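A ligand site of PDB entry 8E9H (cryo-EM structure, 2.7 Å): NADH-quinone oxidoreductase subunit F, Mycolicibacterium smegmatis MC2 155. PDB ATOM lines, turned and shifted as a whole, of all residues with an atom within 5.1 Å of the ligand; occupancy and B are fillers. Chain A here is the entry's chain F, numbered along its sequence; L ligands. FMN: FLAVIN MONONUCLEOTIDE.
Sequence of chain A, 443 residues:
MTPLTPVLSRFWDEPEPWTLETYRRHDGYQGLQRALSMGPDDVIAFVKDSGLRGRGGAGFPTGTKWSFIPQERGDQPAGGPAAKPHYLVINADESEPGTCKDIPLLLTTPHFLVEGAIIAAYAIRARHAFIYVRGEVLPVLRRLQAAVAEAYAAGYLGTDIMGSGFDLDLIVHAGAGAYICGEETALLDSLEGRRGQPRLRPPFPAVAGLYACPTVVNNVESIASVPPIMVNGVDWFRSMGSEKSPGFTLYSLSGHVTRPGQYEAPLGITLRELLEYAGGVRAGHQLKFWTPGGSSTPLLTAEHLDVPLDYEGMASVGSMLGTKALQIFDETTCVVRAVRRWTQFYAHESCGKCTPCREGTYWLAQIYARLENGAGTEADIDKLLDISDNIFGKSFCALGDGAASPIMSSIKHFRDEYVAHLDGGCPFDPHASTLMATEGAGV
O3' of the ligand sits close to OE2 of Glu 184 (3.5 Å).
An oxygen (O2) of the ligand is in hydrogen-bond range of the side-chain amide nitrogen (ND2) of Asn 219, at 2.5 Å.
The backbone NH of Arg 55 is in hydrogen-bond range of an oxygen (O3P) of the ligand.
The side-chain hydroxyl (OG) of Ser 222 is in hydrogen-bond range of an oxygen (O3P) of the ligand (3.0 Å).
N3 of the ligand lies within hydrogen-bond range of O of Asp 93, 2.6 Å away.
ND2 of Asn 91 sits close to N1 of the ligand, at 3.2 Å.
N of Gly 56 sits at hydrogen-bond distance from O3P of the ligand (2.5 Å).
An oxygen (O1P) of the ligand sits close to the side-chain amide nitrogen of Asn 218 (3.2 Å).
NZ of Lys 65 is in salt-bridge range of O2P of the ligand, 2.6 Å away.
The backbone NH (N) of Asn 219 sits at hydrogen-bond distance from an oxygen (O1P) of the ligand (2.4 Å).
ND2 of Asn 91 lies within hydrogen-bond range of O of Gly 182 (2.5 Å).
O of Asn 218 lies within hydrogen-bond range of N of Asn 91, at 2.6 Å.
OD1 of Asn 91 sits close to N of Asp 93 (3.3 Å).
NZ of Lys 65 lies close to ND2 of Asn 218 (3.0 Å).
N of Gly 182 lies within hydrogen-bond range of OD2 of Asp 93 (3.4 Å).
The side-chain carboxylate of Asp 102 sits at hydrogen-bond distance from the side-chain amide nitrogen of Asn 219, at 2.9 Å.
O of Phe 60 lies within hydrogen-bond range of N of Gly 54, at 2.5 Å.
The side-chain hydroxyl (OG) of Ser 222 sits at hydrogen-bond distance from the backbone NH (N) of Arg 55, at 2.7 Å.
The backbone carbonyl oxygen of Gly 182 sits close to a nitrogen (N10) of the ligand, at 3.2 Å.
Residues that only touch the ligand: Gly 54 (2.8 Å), Ala 58 (3.0 Å), Tyr 179 (3.4 Å), Glu 183 (3.5 Å), Val 217 (3.5 Å), Ala 398 (3.5 Å), Ser 95 (3.6 Å), Glu 94 (3.6 Å) and Leu 399 (3.7 Å).
Hydrophobic or aromatic side chains that line the ligand: Ala 58, Tyr 179, Val 217, Ala 398 and Leu 399.
Of the 28 residues printed, 19 come within 4 Å of the ligand.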
ATOM      1  N   ARG A  53      -4.980   3.127   9.631  1.00  0.00           N
ATOM      2  CA  ARG A  53      -6.312   2.612   9.408  1.00  0.00           C
ATOM      3  C   ARG A  53      -6.235   1.260   8.720  1.00  0.00           C
ATOM      4  O   ARG A  53      -5.296   0.983   7.968  1.00  0.00           O
ATOM      5  CB  ARG A  53      -7.153   3.581   8.569  1.00  0.00           C
ATOM      6  CG  ARG A  53      -7.598   4.805   9.323  1.00  0.00           C
ATOM      7  CD  ARG A  53      -8.279   5.799   8.408  1.00  0.00           C
ATOM      8  NE  ARG A  53      -9.579   5.313   7.961  1.00  0.00           N
ATOM      9  CZ  ARG A  53     -10.398   5.995   7.172  1.00  0.00           C
ATOM     10  NH1 ARG A  53     -10.078   7.184   6.701  1.00  0.00           N
ATOM     11  NH2 ARG A  53     -11.570   5.456   6.840  1.00  0.00           N
ATOM     12  N   GLY A  54      -7.228   0.425   8.990  1.00  0.00           N
ATOM     13  CA  GLY A  54      -7.237  -0.940   8.489  1.00  0.00           C
ATOM     14  C   GLY A  54      -6.978  -1.046   7.000  1.00  0.00           C
ATOM     15  O   GLY A  54      -7.685  -0.446   6.197  1.00  0.00           O
ATOM     16  N   ARG A  55      -5.963  -1.835   6.640  1.00  0.00           N
ATOM     17  CA  ARG A  55      -5.631  -2.037   5.242  1.00  0.00           C
ATOM     18  C   ARG A  55      -6.361  -3.231   4.628  1.00  0.00           C
ATOM     19  O   ARG A  55      -6.182  -3.492   3.429  1.00  0.00           O
ATOM     20  CB  ARG A  55      -4.122  -2.234   5.087  1.00  0.00           C
ATOM     21  CG  ARG A  55      -3.303  -1.133   5.719  1.00  0.00           C
ATOM     22  CD  ARG A  55      -3.689   0.225   5.174  1.00  0.00           C
ATOM     23  NE  ARG A  55      -2.691   1.235   5.497  1.00  0.00           N
ATOM     24  CZ  ARG A  55      -2.959   2.449   5.936  1.00  0.00           C
ATOM     25  NH1 ARG A  55      -4.196   2.879   6.105  1.00  0.00           N
ATOM     26  NH2 ARG A  55      -1.957   3.275   6.219  1.00  0.00           N
ATOM     27  N   GLY A  56      -7.151  -3.953   5.407  1.00  0.00           N
ATOM     28  CA  GLY A  56      -7.864  -5.116   4.890  1.00  0.00           C
ATOM     29  C   GLY A  56      -9.133  -4.797   4.148  1.00  0.00           C
ATOM     30  O   GLY A  56      -9.824  -5.722   3.692  1.00  0.00           O
ATOM     31  N   GLY A  57      -9.473  -3.523   4.015  1.00  0.00           N
ATOM     32  CA  GLY A  57     -10.677  -3.085   3.322  1.00  0.00           C
ATOM     33  C   GLY A  57     -11.657  -2.335   4.199  1.00  0.00           C
ATOM     34  O   GLY A  57     -12.334  -1.431   3.703  1.00  0.00           O
ATOM     35  N   ALA A  58     -11.739  -2.667   5.482  1.00  0.00           N
ATOM     36  CA  ALA A  58     -12.645  -1.950   6.371  1.00  0.00           C
ATOM     37  C   ALA A  58     -12.215  -0.508   6.547  1.00  0.00           C
ATOM     38  O   ALA A  58     -13.066   0.393   6.627  1.00  0.00           O
ATOM     39  CB  ALA A  58     -12.721  -2.655   7.728  1.00  0.00           C
ATOM     40  N   PHE A  60     -10.908   0.720   9.188  1.00  0.00           N
ATOM     41  CA  PHE A  60     -11.108   1.136  10.569  1.00  0.00           C
ATOM     42  C   PHE A  60      -9.781   1.509  11.203  1.00  0.00           C
ATOM     43  O   PHE A  60      -8.758   0.872  10.928  1.00  0.00           O
ATOM     44  CB  PHE A  60     -11.759   0.008  11.358  1.00  0.00           C
ATOM     45  CG  PHE A  60     -12.359   0.450  12.655  1.00  0.00           C
ATOM     46  CD1 PHE A  60     -13.599   1.073  12.678  1.00  0.00           C
ATOM     47  CD2 PHE A  60     -11.700   0.228  13.846  1.00  0.00           C
ATOM     48  CE1 PHE A  60     -14.152   1.480  13.878  1.00  0.00           C
ATOM     49  CE2 PHE A  60     -12.253   0.635  15.046  1.00  0.00           C
ATOM     50  CZ  PHE A  60     -13.487   1.265  15.053  1.00  0.00           C
ATOM     51  N   THR A  62      -6.776   1.255  13.326  1.00  0.00           N
ATOM     52  CA  THR A  62      -6.257   0.095  14.053  1.00  0.00           C
ATOM     53  C   THR A  62      -5.982   0.439  15.511  1.00  0.00           C
ATOM     54  O   THR A  62      -6.139  -0.422  16.386  1.00  0.00           O
ATOM     55  CB  THR A  62      -4.979  -0.419  13.386  1.00  0.00           C
ATOM     56  OG1 THR A  62      -3.945   0.565  13.516  1.00  0.00           O
ATOM     57  CG2 THR A  62      -5.228  -0.706  11.918  1.00  0.00           C
ATOM     58  N   LYS A  65      -9.109   0.048  17.456  1.00  0.00           N
ATOM     59  CA  LYS A  65      -9.422  -1.368  17.514  1.00  0.00           C
ATOM     60  C   LYS A  65      -8.623  -2.050  18.615  1.00  0.00           C
ATOM     61  O   LYS A  65      -9.167  -2.838  19.392  1.00  0.00           O
ATOM     62  CB  LYS A  65      -9.160  -2.019  16.157  1.00  0.00           C
ATOM     63  CG  LYS A  65      -9.726  -3.420  16.035  1.00  0.00           C
ATOM     64  CD  LYS A  65      -9.121  -4.170  14.875  1.00  0.00           C
ATOM     65  CE  LYS A  65      -9.508  -3.564  13.548  1.00  0.00           C
ATOM     66  NZ  LYS A  65      -8.855  -4.260  12.413  1.00  0.00           N
ATOM     67  N   ASN A  91      -4.679 -11.456   9.892  1.00  0.00           N
ATOM     68  CA  ASN A  91      -5.467 -11.941   8.764  1.00  0.00           C
ATOM     69  C   ASN A  91      -4.580 -12.015   7.534  1.00  0.00           C
ATOM     70  O   ASN A  91      -4.648 -11.203   6.611  1.00  0.00           O
ATOM     71  CB  ASN A  91      -6.668 -11.037   8.540  1.00  0.00           C
ATOM     72  CG  ASN A  91      -7.667 -11.644   7.592  1.00  0.00           C
ATOM     73  OD1 ASN A  91      -7.413 -12.671   6.978  1.00  0.00           O
ATOM     74  ND2 ASN A  91      -8.820 -11.000   7.458  1.00  0.00           N
ATOM     75  N   ASP A  93      -4.933 -14.115   5.376  1.00  0.00           N
ATOM     76  CA  ASP A  93      -5.785 -14.461   4.255  1.00  0.00           C
ATOM     77  C   ASP A  93      -5.903 -13.270   3.317  1.00  0.00           C
ATOM     78  O   ASP A  93      -6.260 -12.160   3.725  1.00  0.00           O
ATOM     79  CB  ASP A  93      -7.169 -14.885   4.740  1.00  0.00           C
ATOM     80  CG  ASP A  93      -7.955 -15.602   3.680  1.00  0.00           C
ATOM     81  OD1 ASP A  93      -7.698 -15.365   2.481  1.00  0.00           O
ATOM     82  OD2 ASP A  93      -8.837 -16.412   4.045  1.00  0.00           O
ATOM     83  N   GLU A  94      -5.596 -13.494   2.042  1.00  0.00           N
ATOM     84  CA  GLU A  94      -5.722 -12.455   1.018  1.00  0.00           C
ATOM     85  C   GLU A  94      -6.344 -13.144  -0.196  1.00  0.00           C
ATOM     86  O   GLU A  94      -5.635 -13.677  -1.048  1.00  0.00           O
ATOM     87  CB  GLU A  94      -4.382 -11.818   0.691  1.00  0.00           C
ATOM     88  N   SER A  95      -7.671 -13.118  -0.248  1.00  0.00           N
ATOM     89  CA  SER A  95      -8.380 -13.818  -1.307  1.00  0.00           C
ATOM     90  C   SER A  95      -9.389 -12.949  -2.042  1.00  0.00           C
ATOM     91  O   SER A  95     -10.042 -13.446  -2.957  1.00  0.00           O
ATOM     92  CB  SER A  95      -9.098 -15.053  -0.733  1.00  0.00           C
ATOM     93  OG  SER A  95      -9.613 -15.854  -1.779  1.00  0.00           O
ATOM     94  N   GLU A  96      -9.519 -11.680  -1.687  1.00  0.00           N
ATOM     95  CA  GLU A  96     -10.408 -10.812  -2.443  1.00  0.00           C
ATOM     96  C   GLU A  96      -9.861 -10.660  -3.853  1.00  0.00           C
ATOM     97  O   GLU A  96      -8.660 -10.412  -4.027  1.00  0.00           O
ATOM     98  CB  GLU A  96     -10.523  -9.453  -1.775  1.00  0.00           C
ATOM     99  CG  GLU A  96     -11.606  -8.581  -2.384  1.00  0.00           C
ATOM    100  CD  GLU A  96     -11.800  -7.282  -1.642  1.00  0.00           C
ATOM    101  OE1 GLU A  96     -11.523  -7.240  -0.428  1.00  0.00           O
ATOM    102  OE2 GLU A  96     -12.233  -6.289  -2.269  1.00  0.00           O
ATOM    103  N   ASP A 102      -0.811  -8.417  -0.089  1.00  0.00           N
ATOM    104  CA  ASP A 102      -0.352  -9.142   1.094  1.00  0.00           C
ATOM    105  C   ASP A 102       0.648 -10.223   0.712  1.00  0.00           C
ATOM    106  O   ASP A 102       1.695 -10.374   1.362  1.00  0.00           O
ATOM    107  CB  ASP A 102      -1.559  -9.772   1.805  1.00  0.00           C
ATOM    108  CG  ASP A 102      -2.501  -8.736   2.370  1.00  0.00           C
ATOM    109  OD1 ASP A 102      -2.045  -7.623   2.690  1.00  0.00           O
ATOM    110  OD2 ASP A 102      -3.709  -9.030   2.480  1.00  0.00           O
ATOM    111  N   TYR A 179     -12.701 -17.862   0.612  1.00  0.00           N
ATOM    112  CA  TYR A 179     -12.568 -16.416   0.637  1.00  0.00           C
ATOM    113  C   TYR A 179     -13.222 -15.821   1.870  1.00  0.00           C
ATOM    114  O   TYR A 179     -12.664 -14.929   2.512  1.00  0.00           O
ATOM    115  CB  TYR A 179     -13.183 -15.825  -0.634  1.00  0.00           C
ATOM    116  CG  TYR A 179     -13.465 -14.343  -0.558  1.00  0.00           C
ATOM    117  CD1 TYR A 179     -12.483 -13.451  -0.173  1.00  0.00           C
ATOM    118  CD2 TYR A 179     -14.706 -13.841  -0.892  1.00  0.00           C
ATOM    119  CE1 TYR A 179     -12.742 -12.105  -0.100  1.00  0.00           C
ATOM    120  CE2 TYR A 179     -14.971 -12.489  -0.840  1.00  0.00           C
ATOM    121  CZ  TYR A 179     -13.978 -11.626  -0.441  1.00  0.00           C
ATOM    122  OH  TYR A 179     -14.231 -10.283  -0.381  1.00  0.00           O
ATOM    123  N   ILE A 180     -14.405 -16.327   2.231  1.00  0.00           N
ATOM    124  CA  ILE A 180     -15.146 -15.763   3.350  1.00  0.00           C
ATOM    125  C   ILE A 180     -14.335 -15.818   4.634  1.00  0.00           C
ATOM    126  O   ILE A 180     -14.509 -14.989   5.530  1.00  0.00           O
ATOM    127  CB  ILE A 180     -16.500 -16.467   3.511  1.00  0.00           C
ATOM    128  CG1 ILE A 180     -17.286 -15.880   4.675  1.00  0.00           C
ATOM    129  CG2 ILE A 180     -16.295 -17.958   3.738  1.00  0.00           C
ATOM    130  CD1 ILE A 180     -17.501 -14.391   4.571  1.00  0.00           C
ATOM    131  N   GLY A 182     -11.589 -14.844   5.212  1.00  0.00           N
ATOM    132  CA  GLY A 182     -10.873 -13.605   5.431  1.00  0.00           C
ATOM    133  C   GLY A 182     -11.628 -12.568   6.230  1.00  0.00           C
ATOM    134  O   GLY A 182     -11.071 -11.518   6.525  1.00  0.00           O
ATOM    135  N   GLU A 183     -12.878 -12.846   6.581  1.00  0.00           N
ATOM    136  CA  GLU A 183     -13.713 -11.903   7.310  1.00  0.00           C
ATOM    137  C   GLU A 183     -13.702 -12.234   8.797  1.00  0.00           C
ATOM    138  O   GLU A 183     -13.786 -13.407   9.176  1.00  0.00           O
ATOM    139  CB  GLU A 183     -15.143 -11.931   6.764  1.00  0.00           C
ATOM    140  CG  GLU A 183     -16.048 -10.855   7.329  1.00  0.00           C
ATOM    141  CD  GLU A 183     -16.827 -11.318   8.530  1.00  0.00           C
ATOM    142  OE1 GLU A 183     -17.130 -12.521   8.628  1.00  0.00           O
ATOM    143  OE2 GLU A 183     -17.162 -10.468   9.384  1.00  0.00           O
ATOM    144  N   GLU A 184     -13.582 -11.201   9.629  1.00  0.00           N
ATOM    145  CA  GLU A 184     -13.588 -11.388  11.071  1.00  0.00           C
ATOM    146  C   GLU A 184     -14.732 -12.294  11.488  1.00  0.00           C
ATOM    147  O   GLU A 184     -15.818 -12.236  10.916  1.00  0.00           O
ATOM    148  CB  GLU A 184     -13.707 -10.056  11.801  1.00  0.00           C
ATOM    149  CG  GLU A 184     -12.579  -9.095  11.531  1.00  0.00           C
ATOM    150  CD  GLU A 184     -12.627  -7.897  12.457  1.00  0.00           C
ATOM    151  OE1 GLU A 184     -13.445  -7.894  13.393  1.00  0.00           O
ATOM    152  OE2 GLU A 184     -11.845  -6.945  12.242  1.00  0.00           O
ATOM    153  N   VAL A 217      -8.220  -8.802  15.068  1.00  0.00           N
ATOM    154  CA  VAL A 217      -7.941  -9.305  13.729  1.00  0.00           C
ATOM    155  C   VAL A 217      -7.463  -8.128  12.886  1.00  0.00           C
ATOM    156  O   VAL A 217      -8.169  -7.128  12.762  1.00  0.00           O
ATOM    157  CB  VAL A 217      -9.179  -9.960  13.098  1.00  0.00           C
ATOM    158  CG1 VAL A 217      -8.853 -10.505  11.728  1.00  0.00           C
ATOM    159  CG2 VAL A 217      -9.690 -11.070  14.004  1.00  0.00           C
ATOM    160  N   ASN A 218      -6.267  -8.254  12.323  1.00  0.00           N
ATOM    161  CA  ASN A 218      -5.697  -7.198  11.514  1.00  0.00           C
ATOM    162  C   ASN A 218      -5.137  -7.762  10.213  1.00  0.00           C
ATOM    163  O   ASN A 218      -4.579  -8.866  10.197  1.00  0.00           O
ATOM    164  CB  ASN A 218      -4.591  -6.450  12.252  1.00  0.00           C
ATOM    165  CG  ASN A 218      -5.128  -5.497  13.281  1.00  0.00           C
ATOM    166  OD1 ASN A 218      -4.851  -5.634  14.477  1.00  0.00           O
ATOM    167  ND2 ASN A 218      -5.894  -4.515  12.835  1.00  0.00           N
ATOM    168  N   ASN A 219      -5.287  -7.000   9.136  1.00  0.00           N
ATOM    169  CA  ASN A 219      -4.676  -7.373   7.874  1.00  0.00           C
ATOM    170  C   ASN A 219      -3.164  -7.303   7.990  1.00  0.00           C
ATOM    171  O   ASN A 219      -2.619  -6.496   8.751  1.00  0.00           O
ATOM    172  CB  ASN A 219      -5.159  -6.446   6.757  1.00  0.00           C
ATOM    173  CG  ASN A 219      -4.506  -6.744   5.432  1.00  0.00           C
ATOM    174  OD1 ASN A 219      -3.866  -5.878   4.842  1.00  0.00           O
ATOM    175  ND2 ASN A 219      -4.668  -7.961   4.958  1.00  0.00           N
ATOM    176  N   VAL A 220      -2.477  -8.162   7.234  1.00  0.00           N
ATOM    177  CA  VAL A 220      -1.020  -8.187   7.324  1.00  0.00           C
ATOM    178  C   VAL A 220      -0.430  -6.839   6.948  1.00  0.00           C
ATOM    179  O   VAL A 220       0.602  -6.438   7.491  1.00  0.00           O
ATOM    180  CB  VAL A 220      -0.443  -9.313   6.446  1.00  0.00           C
ATOM    181  CG1 VAL A 220      -0.871 -10.657   6.978  1.00  0.00           C
ATOM    182  CG2 VAL A 220      -0.876  -9.150   5.009  1.00  0.00           C
ATOM    183  N   SER A 222      -1.794  -3.870   7.592  1.00  0.00           N
ATOM    184  CA  SER A 222      -1.957  -3.003   8.749  1.00  0.00           C
ATOM    185  C   SER A 222      -0.880  -3.275   9.781  1.00  0.00           C
ATOM    186  O   SER A 222      -0.230  -2.350  10.273  1.00  0.00           O
ATOM    187  CB  SER A 222      -3.345  -3.205   9.353  1.00  0.00           C
ATOM    188  OG  SER A 222      -4.353  -3.154   8.361  1.00  0.00           O
ATOM    189  N   CYS A 397     -23.274 -10.801   6.348  1.00  0.00           N
ATOM    190  CA  CYS A 397     -21.960 -10.174   6.381  1.00  0.00           C
ATOM    191  C   CYS A 397     -21.775  -9.362   5.113  1.00  0.00           C
ATOM    192  O   CYS A 397     -22.649  -9.324   4.237  1.00  0.00           O
ATOM    193  CB  CYS A 397     -20.828 -11.197   6.513  1.00  0.00           C
ATOM    194  SG  CYS A 397     -20.315 -11.938   4.961  1.00  0.00           S
ATOM    195  N   ALA A 398     -20.629  -8.703   5.017  1.00  0.00           N
ATOM    196  CA  ALA A 398     -20.383  -7.786   3.913  1.00  0.00           C
ATOM    197  C   ALA A 398     -20.082  -8.492   2.596  1.00  0.00           C
ATOM    198  O   ALA A 398     -19.942  -7.804   1.588  1.00  0.00           O
ATOM    199  CB  ALA A 398     -19.234  -6.849   4.270  1.00  0.00           C
ATOM    200  N   LEU A 399     -19.973  -9.817   2.575  1.00  0.00           N
ATOM    201  CA  LEU A 399     -19.727 -10.489   1.305  1.00  0.00           C
ATOM    202  C   LEU A 399     -20.907 -10.306   0.350  1.00  0.00           C
ATOM    203  O   LEU A 399     -20.710 -10.180  -0.858  1.00  0.00           O
ATOM    204  CB  LEU A 399     -19.462 -11.966   1.517  1.00  0.00           C
ATOM    205  CG  LEU A 399     -18.945 -12.688   0.276  1.00  0.00           C
ATOM    206  CD1 LEU A 399     -17.919 -13.745   0.640  1.00  0.00           C
ATOM    207  CD2 LEU A 399     -20.083 -13.321  -0.507  1.00  0.00           C
HETATM  208  N1  FMN L   1      -9.222  -8.630   5.386  1.00  0.00           N
HETATM  209  C2  FMN L   1      -7.951  -9.106   5.116  1.00  0.00           C
HETATM  210  O2  FMN L   1      -6.976  -8.570   5.653  1.00  0.00           O
HETATM  211  N3  FMN L   1      -7.766 -10.155   4.249  1.00  0.00           N
HETATM  212  C4  FMN L   1      -8.853 -10.748   3.657  1.00  0.00           C
HETATM  213  O4  FMN L   1      -8.707 -11.692   2.882  1.00  0.00           O
HETATM  214  C4A FMN L   1     -10.128 -10.284   3.920  1.00  0.00           C
HETATM  215  N5  FMN L   1     -11.205 -10.878   3.325  1.00  0.00           N
HETATM  216  C5A FMN L   1     -12.480 -10.414   3.588  1.00  0.00           C
HETATM  217  C6  FMN L   1     -13.556 -11.023   2.974  1.00  0.00           C
HETATM  218  C7  FMN L   1     -14.842 -10.574   3.211  1.00  0.00           C
HETATM  219  C7M FMN L   1     -15.985 -11.276   2.532  1.00  0.00           C
HETATM  220  C8  FMN L   1     -15.042  -9.511   4.091  1.00  0.00           C
HETATM  221  C8M FMN L   1     -16.401  -8.982   4.394  1.00  0.00           C
HETATM  222  C9  FMN L   1     -13.953  -8.902   4.712  1.00  0.00           C
HETATM  223  C9A FMN L   1     -12.665  -9.355   4.452  1.00  0.00           C
HETATM  224  N10 FMN L   1     -11.574  -8.751   5.051  1.00  0.00           N
HETATM  225  C10 FMN L   1     -10.308  -9.213   4.792  1.00  0.00           C
HETATM  226  C1' FMN L   1     -11.722  -7.600   6.014  1.00  0.00           C
HETATM  227  C2' FMN L   1     -11.807  -8.163   7.410  1.00  0.00           C
HETATM  228  O2' FMN L   1     -13.084  -7.897   7.932  1.00  0.00           O
HETATM  229  C3' FMN L   1     -10.711  -7.601   8.320  1.00  0.00           C
HETATM  230  O3' FMN L   1     -10.534  -8.462   9.419  1.00  0.00           O
HETATM  231  C4' FMN L   1     -11.048  -6.204   8.825  1.00  0.00           C
HETATM  232  O4' FMN L   1     -11.343  -5.365   7.732  1.00  0.00           O
HETATM  233  C5' FMN L   1      -9.894  -5.612   9.610  1.00  0.00           C
HETATM  234  O5' FMN L   1      -8.808  -5.390   8.745  1.00  0.00           O
HETATM  235  P   FMN L   1      -7.681  -4.308   9.102  1.00  0.00           P
HETATM  236  O1P FMN L   1      -6.516  -5.000   9.753  1.00  0.00           O
HETATM  237  O2P FMN L   1      -8.244  -3.287  10.062  1.00  0.00           O
HETATM  238  O3P FMN L   1      -7.217  -3.656   7.839  1.00  0.00           O
